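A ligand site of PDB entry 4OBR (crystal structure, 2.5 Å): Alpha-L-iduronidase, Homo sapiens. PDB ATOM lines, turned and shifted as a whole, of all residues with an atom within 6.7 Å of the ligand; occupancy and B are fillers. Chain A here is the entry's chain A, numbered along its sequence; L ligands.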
ATOM      1  N   GLY A  25      25.066  -3.775 -13.831  1.00  0.00           N
ATOM      2  CA  GLY A  25      23.624  -3.744 -13.988  1.00  0.00           C
ATOM      3  C   GLY A  25      23.127  -4.384 -15.268  1.00  0.00           C
ATOM      4  O   GLY A  25      23.916  -4.797 -16.124  1.00  0.00           O
ATOM      5  N   PHE A  26      21.806  -4.483 -15.399  1.00  0.00           N
ATOM      6  CA  PHE A  26      21.203  -5.042 -16.598  1.00  0.00           C
ATOM      7  C   PHE A  26      19.696  -4.812 -16.642  1.00  0.00           C
ATOM      8  O   PHE A  26      19.065  -4.412 -15.652  1.00  0.00           O
ATOM      9  CB  PHE A  26      21.479  -6.544 -16.695  1.00  0.00           C
ATOM     10  CG  PHE A  26      20.711  -7.347 -15.700  1.00  0.00           C
ATOM     11  CD1 PHE A  26      21.145  -7.441 -14.388  1.00  0.00           C
ATOM     12  CD2 PHE A  26      19.549  -8.004 -16.064  1.00  0.00           C
ATOM     13  CE1 PHE A  26      20.434  -8.184 -13.455  1.00  0.00           C
ATOM     14  CE2 PHE A  26      18.832  -8.749 -15.144  1.00  0.00           C
ATOM     15  CZ  PHE A  26      19.282  -8.847 -13.838  1.00  0.00           C
ATOM     16  N   CYS A  27      19.145  -5.113 -17.817  1.00  0.00           N
ATOM     17  CA  CYS A  27      17.723  -5.008 -18.108  1.00  0.00           C
ATOM     18  C   CYS A  27      17.218  -6.381 -18.551  1.00  0.00           C
ATOM     19  O   CYS A  27      17.743  -6.926 -19.524  1.00  0.00           O
ATOM     20  CB  CYS A  27      17.498  -4.002 -19.227  1.00  0.00           C
ATOM     21  SG  CYS A  27      15.761  -3.796 -19.704  1.00  0.00           S
ATOM     22  N   ARG A  63      22.468  -3.037 -10.492  1.00  0.00           N
ATOM     23  CA  ARG A  63      21.395  -2.119 -10.831  1.00  0.00           C
ATOM     24  C   ARG A  63      20.493  -2.794 -11.856  1.00  0.00           C
ATOM     25  O   ARG A  63      20.897  -3.033 -12.985  1.00  0.00           O
ATOM     26  CB  ARG A  63      21.972  -0.815 -11.372  1.00  0.00           C
ATOM     27  CG  ARG A  63      20.922   0.230 -11.667  1.00  0.00           C
ATOM     28  CD  ARG A  63      21.584   1.583 -11.917  1.00  0.00           C
ATOM     29  NE  ARG A  63      20.656   2.527 -12.508  1.00  0.00           N
ATOM     30  CZ  ARG A  63      20.406   2.631 -13.816  1.00  0.00           C
ATOM     31  NH1 ARG A  63      21.008   1.839 -14.691  1.00  0.00           N
ATOM     32  NH2 ARG A  63      19.536   3.548 -14.243  1.00  0.00           N
ATOM     33  N   HIS A  65      16.720  -3.186 -13.877  1.00  0.00           N
ATOM     34  CA  HIS A  65      15.474  -2.544 -14.356  1.00  0.00           C
ATOM     35  C   HIS A  65      14.226  -3.389 -14.040  1.00  0.00           C
ATOM     36  O   HIS A  65      14.312  -4.554 -13.694  1.00  0.00           O
ATOM     37  CB  HIS A  65      15.507  -2.283 -15.875  1.00  0.00           C
ATOM     38  CG  HIS A  65      16.544  -1.292 -16.327  1.00  0.00           C
ATOM     39  ND1 HIS A  65      17.327  -0.567 -15.459  1.00  0.00           N
ATOM     40  CD2 HIS A  65      16.896  -0.899 -17.573  1.00  0.00           C
ATOM     41  CE1 HIS A  65      18.127   0.228 -16.142  1.00  0.00           C
ATOM     42  NE2 HIS A  65      17.888   0.049 -17.427  1.00  0.00           N
ATOM     43  N   GLU A 105      15.863   0.303  -8.735  1.00  0.00           N
ATOM     44  CA  GLU A 105      15.075   1.294  -9.478  1.00  0.00           C
ATOM     45  C   GLU A 105      13.590   1.040  -9.233  1.00  0.00           C
ATOM     46  O   GLU A 105      13.133  -0.077  -9.364  1.00  0.00           O
ATOM     47  CB  GLU A 105      15.374   1.238 -10.972  1.00  0.00           C
ATOM     48  CG  GLU A 105      16.808   1.590 -11.307  1.00  0.00           C
ATOM     49  CD  GLU A 105      17.169   1.186 -12.716  1.00  0.00           C
ATOM     50  OE1 GLU A 105      17.394  -0.022 -12.943  1.00  0.00           O
ATOM     51  OE2 GLU A 105      17.227   2.062 -13.592  1.00  0.00           O
ATOM     52  N   ASN A 155      14.249   4.361 -14.728  1.00  0.00           N
ATOM     53  CA  ASN A 155      15.384   4.608 -15.628  1.00  0.00           C
ATOM     54  C   ASN A 155      15.063   5.512 -16.801  1.00  0.00           C
ATOM     55  O   ASN A 155      14.005   5.391 -17.407  1.00  0.00           O
ATOM     56  CB  ASN A 155      15.933   3.285 -16.190  1.00  0.00           C
ATOM     57  CG  ASN A 155      17.232   3.480 -16.960  1.00  0.00           C
ATOM     58  OD1 ASN A 155      18.212   4.016 -16.433  1.00  0.00           O
ATOM     59  ND2 ASN A 155      17.246   3.040 -18.230  1.00  0.00           N
ATOM     60  N   GLU A 156      16.001   6.395 -17.135  1.00  0.00           N
ATOM     61  CA  GLU A 156      15.925   7.243 -18.330  1.00  0.00           C
ATOM     62  C   GLU A 156      14.512   7.787 -18.609  1.00  0.00           C
ATOM     63  O   GLU A 156      13.918   7.486 -19.649  1.00  0.00           O
ATOM     64  CB  GLU A 156      16.516   6.501 -19.548  1.00  0.00           C
ATOM     65  CG  GLU A 156      18.034   6.317 -19.459  1.00  0.00           C
ATOM     66  CD  GLU A 156      18.648   5.575 -20.633  1.00  0.00           C
ATOM     67  OE1 GLU A 156      17.924   5.217 -21.601  1.00  0.00           O
ATOM     68  OE2 GLU A 156      19.877   5.331 -20.582  1.00  0.00           O
ATOM     69  N   HIS A 159      13.880   9.222 -22.007  1.00  0.00           N
ATOM     70  CA  HIS A 159      13.935   8.288 -23.156  1.00  0.00           C
ATOM     71  C   HIS A 159      12.627   7.500 -23.340  1.00  0.00           C
ATOM     72  O   HIS A 159      12.631   6.399 -23.897  1.00  0.00           O
ATOM     73  CB  HIS A 159      15.150   7.365 -23.055  1.00  0.00           C
ATOM     74  CG  HIS A 159      16.441   8.045 -23.386  1.00  0.00           C
ATOM     75  ND1 HIS A 159      16.976   9.049 -22.600  1.00  0.00           N
ATOM     76  CD2 HIS A 159      17.306   7.872 -24.419  1.00  0.00           C
ATOM     77  CE1 HIS A 159      18.102   9.467 -23.144  1.00  0.00           C
ATOM     78  NE2 HIS A 159      18.336   8.768 -24.237  1.00  0.00           N
ATOM     79  N   HIS A 236      23.633   9.362 -16.892  1.00  0.00           N
ATOM     80  CA  HIS A 236      24.240   8.377 -17.792  1.00  0.00           C
ATOM     81  C   HIS A 236      24.974   9.114 -18.858  1.00  0.00           C
ATOM     82  O   HIS A 236      24.363   9.924 -19.561  1.00  0.00           O
ATOM     83  CB  HIS A 236      23.208   7.533 -18.538  1.00  0.00           C
ATOM     84  CG  HIS A 236      22.258   6.793 -17.658  1.00  0.00           C
ATOM     85  ND1 HIS A 236      22.567   6.398 -16.364  1.00  0.00           N
ATOM     86  CD2 HIS A 236      21.017   6.333 -17.911  1.00  0.00           C
ATOM     87  CE1 HIS A 236      21.532   5.749 -15.861  1.00  0.00           C
ATOM     88  NE2 HIS A 236      20.586   5.689 -16.779  1.00  0.00           N
ATOM     89  N   LYS A 238      28.000   7.974 -21.913  1.00  0.00           N
ATOM     90  CA  LYS A 238      28.761   6.893 -22.535  1.00  0.00           C
ATOM     91  C   LYS A 238      29.760   7.456 -23.523  1.00  0.00           C
ATOM     92  O   LYS A 238      29.551   8.533 -24.084  1.00  0.00           O
ATOM     93  CB  LYS A 238      27.820   5.906 -23.225  1.00  0.00           C
ATOM     94  CG  LYS A 238      26.531   5.672 -22.447  1.00  0.00           C
ATOM     95  CD  LYS A 238      25.974   4.276 -22.648  1.00  0.00           C
ATOM     96  CE  LYS A 238      24.754   4.029 -21.766  1.00  0.00           C
ATOM     97  NZ  LYS A 238      24.539   2.579 -21.488  1.00  0.00           N
ATOM     98  N   GLU A 273      25.577   4.345 -15.666  1.00  0.00           N
ATOM     99  CA  GLU A 273      25.776   3.618 -16.926  1.00  0.00           C
ATOM    100  C   GLU A 273      26.936   4.245 -17.697  1.00  0.00           C
ATOM    101  O   GLU A 273      26.731   4.987 -18.637  1.00  0.00           O
ATOM    102  CB  GLU A 273      24.511   3.590 -17.779  1.00  0.00           C
ATOM    103  CG  GLU A 273      23.398   2.709 -17.223  1.00  0.00           C
ATOM    104  CD  GLU A 273      22.186   2.611 -18.153  1.00  0.00           C
ATOM    105  OE1 GLU A 273      22.363   2.829 -19.372  1.00  0.00           O
ATOM    106  OE2 GLU A 273      21.063   2.325 -17.649  1.00  0.00           O
ATOM    107  N   ASP A 275      29.370   3.233 -19.808  1.00  0.00           N
ATOM    108  CA  ASP A 275      29.910   2.260 -20.758  1.00  0.00           C
ATOM    109  C   ASP A 275      30.667   2.941 -21.904  1.00  0.00           C
ATOM    110  O   ASP A 275      30.278   4.029 -22.343  1.00  0.00           O
ATOM    111  CB  ASP A 275      28.770   1.401 -21.293  1.00  0.00           C
ATOM    112  CG  ASP A 275      27.891   0.856 -20.165  1.00  0.00           C
ATOM    113  OD1 ASP A 275      28.393  -0.003 -19.393  1.00  0.00           O
ATOM    114  OD2 ASP A 275      26.722   1.276 -20.046  1.00  0.00           O
ATOM    115  N   LEU A 277      30.563   2.327 -24.984  1.00  0.00           N
ATOM    116  CA  LEU A 277      29.717   2.435 -26.159  1.00  0.00           C
ATOM    117  C   LEU A 277      28.282   2.016 -25.861  1.00  0.00           C
ATOM    118  O   LEU A 277      28.031   0.943 -25.296  1.00  0.00           O
ATOM    119  CB  LEU A 277      30.266   1.537 -27.286  1.00  0.00           C
ATOM    120  CG  LEU A 277      29.433   1.400 -28.560  1.00  0.00           C
ATOM    121  CD1 LEU A 277      29.291   2.755 -29.254  1.00  0.00           C
ATOM    122  CD2 LEU A 277      30.049   0.373 -29.490  1.00  0.00           C
ATOM    123  N   VAL A 278      27.335   2.849 -26.275  1.00  0.00           N
ATOM    124  CA  VAL A 278      25.911   2.537 -26.204  1.00  0.00           C
ATOM    125  C   VAL A 278      25.569   1.283 -27.035  1.00  0.00           C
ATOM    126  O   VAL A 278      26.224   1.000 -28.050  1.00  0.00           O
ATOM    127  CB  VAL A 278      25.044   3.738 -26.652  1.00  0.00           C
ATOM    128  CG1 VAL A 278      25.174   4.000 -28.151  1.00  0.00           C
ATOM    129  CG2 VAL A 278      23.588   3.552 -26.234  1.00  0.00           C
ATOM    130  N   GLY A 279      24.561   0.533 -26.602  1.00  0.00           N
ATOM    131  CA  GLY A 279      24.101  -0.668 -27.317  1.00  0.00           C
ATOM    132  C   GLY A 279      24.806  -1.941 -26.884  1.00  0.00           C
ATOM    133  O   GLY A 279      25.775  -2.370 -27.520  1.00  0.00           O
ATOM    134  N   TRP A 280      24.297  -2.566 -25.836  1.00  0.00           N
ATOM    135  CA  TRP A 280      24.977  -3.705 -25.192  1.00  0.00           C
ATOM    136  C   TRP A 280      25.062  -4.953 -26.068  1.00  0.00           C
ATOM    137  O   TRP A 280      26.057  -5.673 -26.021  1.00  0.00           O
ATOM    138  CB  TRP A 280      24.301  -4.048 -23.859  1.00  0.00           C
ATOM    139  CG  TRP A 280      23.056  -4.883 -23.979  1.00  0.00           C
ATOM    140  CD1 TRP A 280      21.770  -4.438 -24.060  1.00  0.00           C
ATOM    141  CD2 TRP A 280      22.992  -6.313 -24.063  1.00  0.00           C
ATOM    142  NE1 TRP A 280      20.902  -5.497 -24.169  1.00  0.00           N
ATOM    143  CE2 TRP A 280      21.621  -6.661 -24.173  1.00  0.00           C
ATOM    144  CE3 TRP A 280      23.948  -7.336 -24.040  1.00  0.00           C
ATOM    145  CZ2 TRP A 280      21.194  -7.982 -24.277  1.00  0.00           C
ATOM    146  CZ3 TRP A 280      23.519  -8.652 -24.136  1.00  0.00           C
ATOM    147  CH2 TRP A 280      22.153  -8.965 -24.260  1.00  0.00           C
ATOM    148  N   SER A 281      24.020  -5.213 -26.857  1.00  0.00           N
ATOM    149  CA  SER A 281      23.943  -6.422 -27.668  1.00  0.00           C
ATOM    150  C   SER A 281      24.600  -6.299 -29.035  1.00  0.00           C
ATOM    151  O   SER A 281      24.630  -7.271 -29.782  1.00  0.00           O
ATOM    152  CB  SER A 281      22.479  -6.843 -27.830  1.00  0.00           C
ATOM    153  OG  SER A 281      21.745  -5.866 -28.524  1.00  0.00           O
ATOM    154  N   ARG A 287      34.903  -6.149 -27.080  1.00  0.00           N
ATOM    155  CA  ARG A 287      34.156  -6.546 -25.888  1.00  0.00           C
ATOM    156  C   ARG A 287      34.434  -7.967 -25.438  1.00  0.00           C
ATOM    157  O   ARG A 287      34.066  -8.343 -24.327  1.00  0.00           O
ATOM    158  CB  ARG A 287      32.655  -6.381 -26.113  1.00  0.00           C
ATOM    159  CG  ARG A 287      32.198  -4.939 -25.992  1.00  0.00           C
ATOM    160  CD  ARG A 287      30.754  -4.765 -26.421  1.00  0.00           C
ATOM    161  NE  ARG A 287      30.284  -3.403 -26.161  1.00  0.00           N
ATOM    162  CZ  ARG A 287      29.104  -2.926 -26.532  1.00  0.00           C
ATOM    163  NH1 ARG A 287      28.247  -3.680 -27.209  1.00  0.00           N
ATOM    164  NH2 ARG A 287      28.771  -1.677 -26.216  1.00  0.00           N
ATOM    165  N   ASP A 323      27.344  -1.140 -17.081  1.00  0.00           N
ATOM    166  CA  ASP A 323      26.055  -1.837 -17.153  1.00  0.00           C
ATOM    167  C   ASP A 323      26.190  -3.145 -17.957  1.00  0.00           C
ATOM    168  O   ASP A 323      25.664  -3.256 -19.058  1.00  0.00           O
ATOM    169  CB  ASP A 323      25.013  -0.909 -17.794  1.00  0.00           C
ATOM    170  CG  ASP A 323      23.582  -1.232 -17.377  1.00  0.00           C
ATOM    171  OD1 ASP A 323      23.326  -1.490 -16.181  1.00  0.00           O
ATOM    172  OD2 ASP A 323      22.700  -1.212 -18.255  1.00  0.00           O
ATOM    173  N   ASN A 324      26.901  -4.122 -17.385  1.00  0.00           N
ATOM    174  CA  ASN A 324      27.347  -5.292 -18.170  1.00  0.00           C
ATOM    175  C   ASN A 324      27.057  -6.648 -17.514  1.00  0.00           C
ATOM    176  O   ASN A 324      27.816  -7.608 -17.662  1.00  0.00           O
ATOM    177  CB  ASN A 324      28.835  -5.155 -18.503  1.00  0.00           C
ATOM    178  CG  ASN A 324      29.701  -4.954 -17.274  1.00  0.00           C
ATOM    179  OD1 ASN A 324      29.233  -5.108 -16.154  1.00  0.00           O
ATOM    180  ND2 ASN A 324      30.962  -4.595 -17.482  1.00  0.00           N
ATOM    181  N   PHE A 326      24.339  -8.304 -18.309  1.00  0.00           N
ATOM    182  CA  PHE A 326      23.505  -8.990 -19.284  1.00  0.00           C
ATOM    183  C   PHE A 326      24.069 -10.390 -19.572  1.00  0.00           C
ATOM    184  O   PHE A 326      25.261 -10.629 -19.391  1.00  0.00           O
ATOM    185  CB  PHE A 326      23.460  -8.217 -20.607  1.00  0.00           C
ATOM    186  CG  PHE A 326      22.769  -6.886 -20.510  1.00  0.00           C
ATOM    187  CD1 PHE A 326      21.403  -6.791 -20.716  1.00  0.00           C
ATOM    188  CD2 PHE A 326      23.494  -5.734 -20.259  1.00  0.00           C
ATOM    189  CE1 PHE A 326      20.764  -5.567 -20.652  1.00  0.00           C
ATOM    190  CE2 PHE A 326      22.868  -4.502 -20.186  1.00  0.00           C
ATOM    191  CZ  PHE A 326      21.495  -4.414 -20.388  1.00  0.00           C
ATOM    192  N   ARG A 337      28.303  -6.920 -24.558  1.00  0.00           N
ATOM    193  CA  ARG A 337      28.724  -6.178 -23.351  1.00  0.00           C
ATOM    194  C   ARG A 337      28.278  -6.888 -22.064  1.00  0.00           C
ATOM    195  O   ARG A 337      27.309  -6.486 -21.393  1.00  0.00           O
ATOM    196  CB  ARG A 337      28.237  -4.731 -23.357  1.00  0.00           C
ATOM    197  CG  ARG A 337      28.940  -3.874 -22.300  1.00  0.00           C
ATOM    198  CD  ARG A 337      27.986  -2.882 -21.646  1.00  0.00           C
ATOM    199  NE  ARG A 337      27.614  -1.803 -22.556  1.00  0.00           N
ATOM    200  CZ  ARG A 337      26.451  -1.157 -22.552  1.00  0.00           C
ATOM    201  NH1 ARG A 337      26.226  -0.186 -23.434  1.00  0.00           N
ATOM    202  NH2 ARG A 337      25.499  -1.472 -21.677  1.00  0.00           N
HETATM  203  C1  LIG L   1      20.225   2.241 -21.570  1.00  0.00           C
HETATM  204  C2  LIG L   1      19.656   1.132 -20.678  1.00  0.00           C
HETATM  205  C3  LIG L   1      20.614  -0.015 -20.268  1.00  0.00           C
HETATM  206  C4  LIG L   1      21.648  -0.421 -21.339  1.00  0.00           C
HETATM  207  C5  LIG L   1      21.632   0.544 -22.550  1.00  0.00           C
HETATM  208  C6  LIG L   1      22.669   0.050 -23.549  1.00  0.00           C
HETATM  209  O1  LIG L   1      19.353   2.538 -22.657  1.00  0.00           O
HETATM  210  O2  LIG L   1      19.177   1.746 -19.477  1.00  0.00           O
HETATM  211  O3  LIG L   1      19.802  -1.137 -19.897  1.00  0.00           O
HETATM  212  O4  LIG L   1      22.965  -0.411 -20.745  1.00  0.00           O
HETATM  213  O5  LIG L   1      21.456   1.904 -22.161  1.00  0.00           O
HETATM  214  O6  LIG L   1      22.477  -0.988 -24.222  1.00  0.00           O
HETATM  215  O7  LIG L   1      23.703   0.768 -23.664  1.00  0.00           O
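Residues that only touch the ligand: Cys 27, Val 278 and Phe 326.
Hydrophobic or aromatic side chains within 4 Å of the ligand: His 65, Val 278, Trp 280 and Phe 326.
The side-chain carboxylate (OD2) of Asp 323 is in hydrogen-bond range of an oxygen (O4) of the ligand (2.6 Å).
The side-chain amide nitrogen of Asn 155 lies within hydrogen-bond range of an oxygen (O2) of the ligand (2.6 Å).
The side-chain carboxylate of Glu 273 lies within hydrogen-bond range of an oxygen (O2) of the ligand.
NH1 of Arg 337 lies within salt-bridge range of O7 of the ligand, at 2.7 Å.
O6 of the ligand is in hydrogen-bond range of N of Trp 280 (2.9 Å).
The side-chain amino group of Lys 238 lies within salt-bridge range of an oxygen (O7) of the ligand, 3.0 Å away.
A ring nitrogen (NE2) of His 65 is in hydrogen-bond range of an oxygen (O2) of the ligand (3.0 Å).
N of Gly 279 is in hydrogen-bond range of O7 of the ligand, 3.1 Å away.
An oxygen (O1) of the ligand sits at hydrogen-bond distance from the side-chain carboxylate (OE1) of Glu 156 (3.2 Å).
OD1 of Asp 323 lies within hydrogen-bond range of N of Phe 26 (3.4 Å).
A ring nitrogen (NE2) of His 65 lies within hydrogen-bond range of the side-chain amide nitrogen of Asn 155, at 3.2 Å.
The side-chain amino group of Lys 238 lies within salt-bridge range of the side-chain carboxylate of Glu 273 (3.0 Å).
The backbone NH (N) of Arg 337 is in hydrogen-bond range of the backbone carbonyl oxygen (O) of Trp 280 (3.0 Å).
The side-chain carboxylate of Asp 275 lies within salt-bridge range of the guanidinium group of Arg 337 (3.4 Å).
The backbone carbonyl oxygen (O) of Leu 277 is in hydrogen-bond range of the guanidinium group (NH1) of Arg 337 (2.8 Å).
The guanidinium group (NH1) of Arg 287 is in hydrogen-bond range of the backbone carbonyl oxygen (O) of Trp 280, at 3.2 Å.
The backbone carbonyl oxygen of Gly 279 lies within hydrogen-bond range of the guanidinium group of Arg 287, 2.8 Å away.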
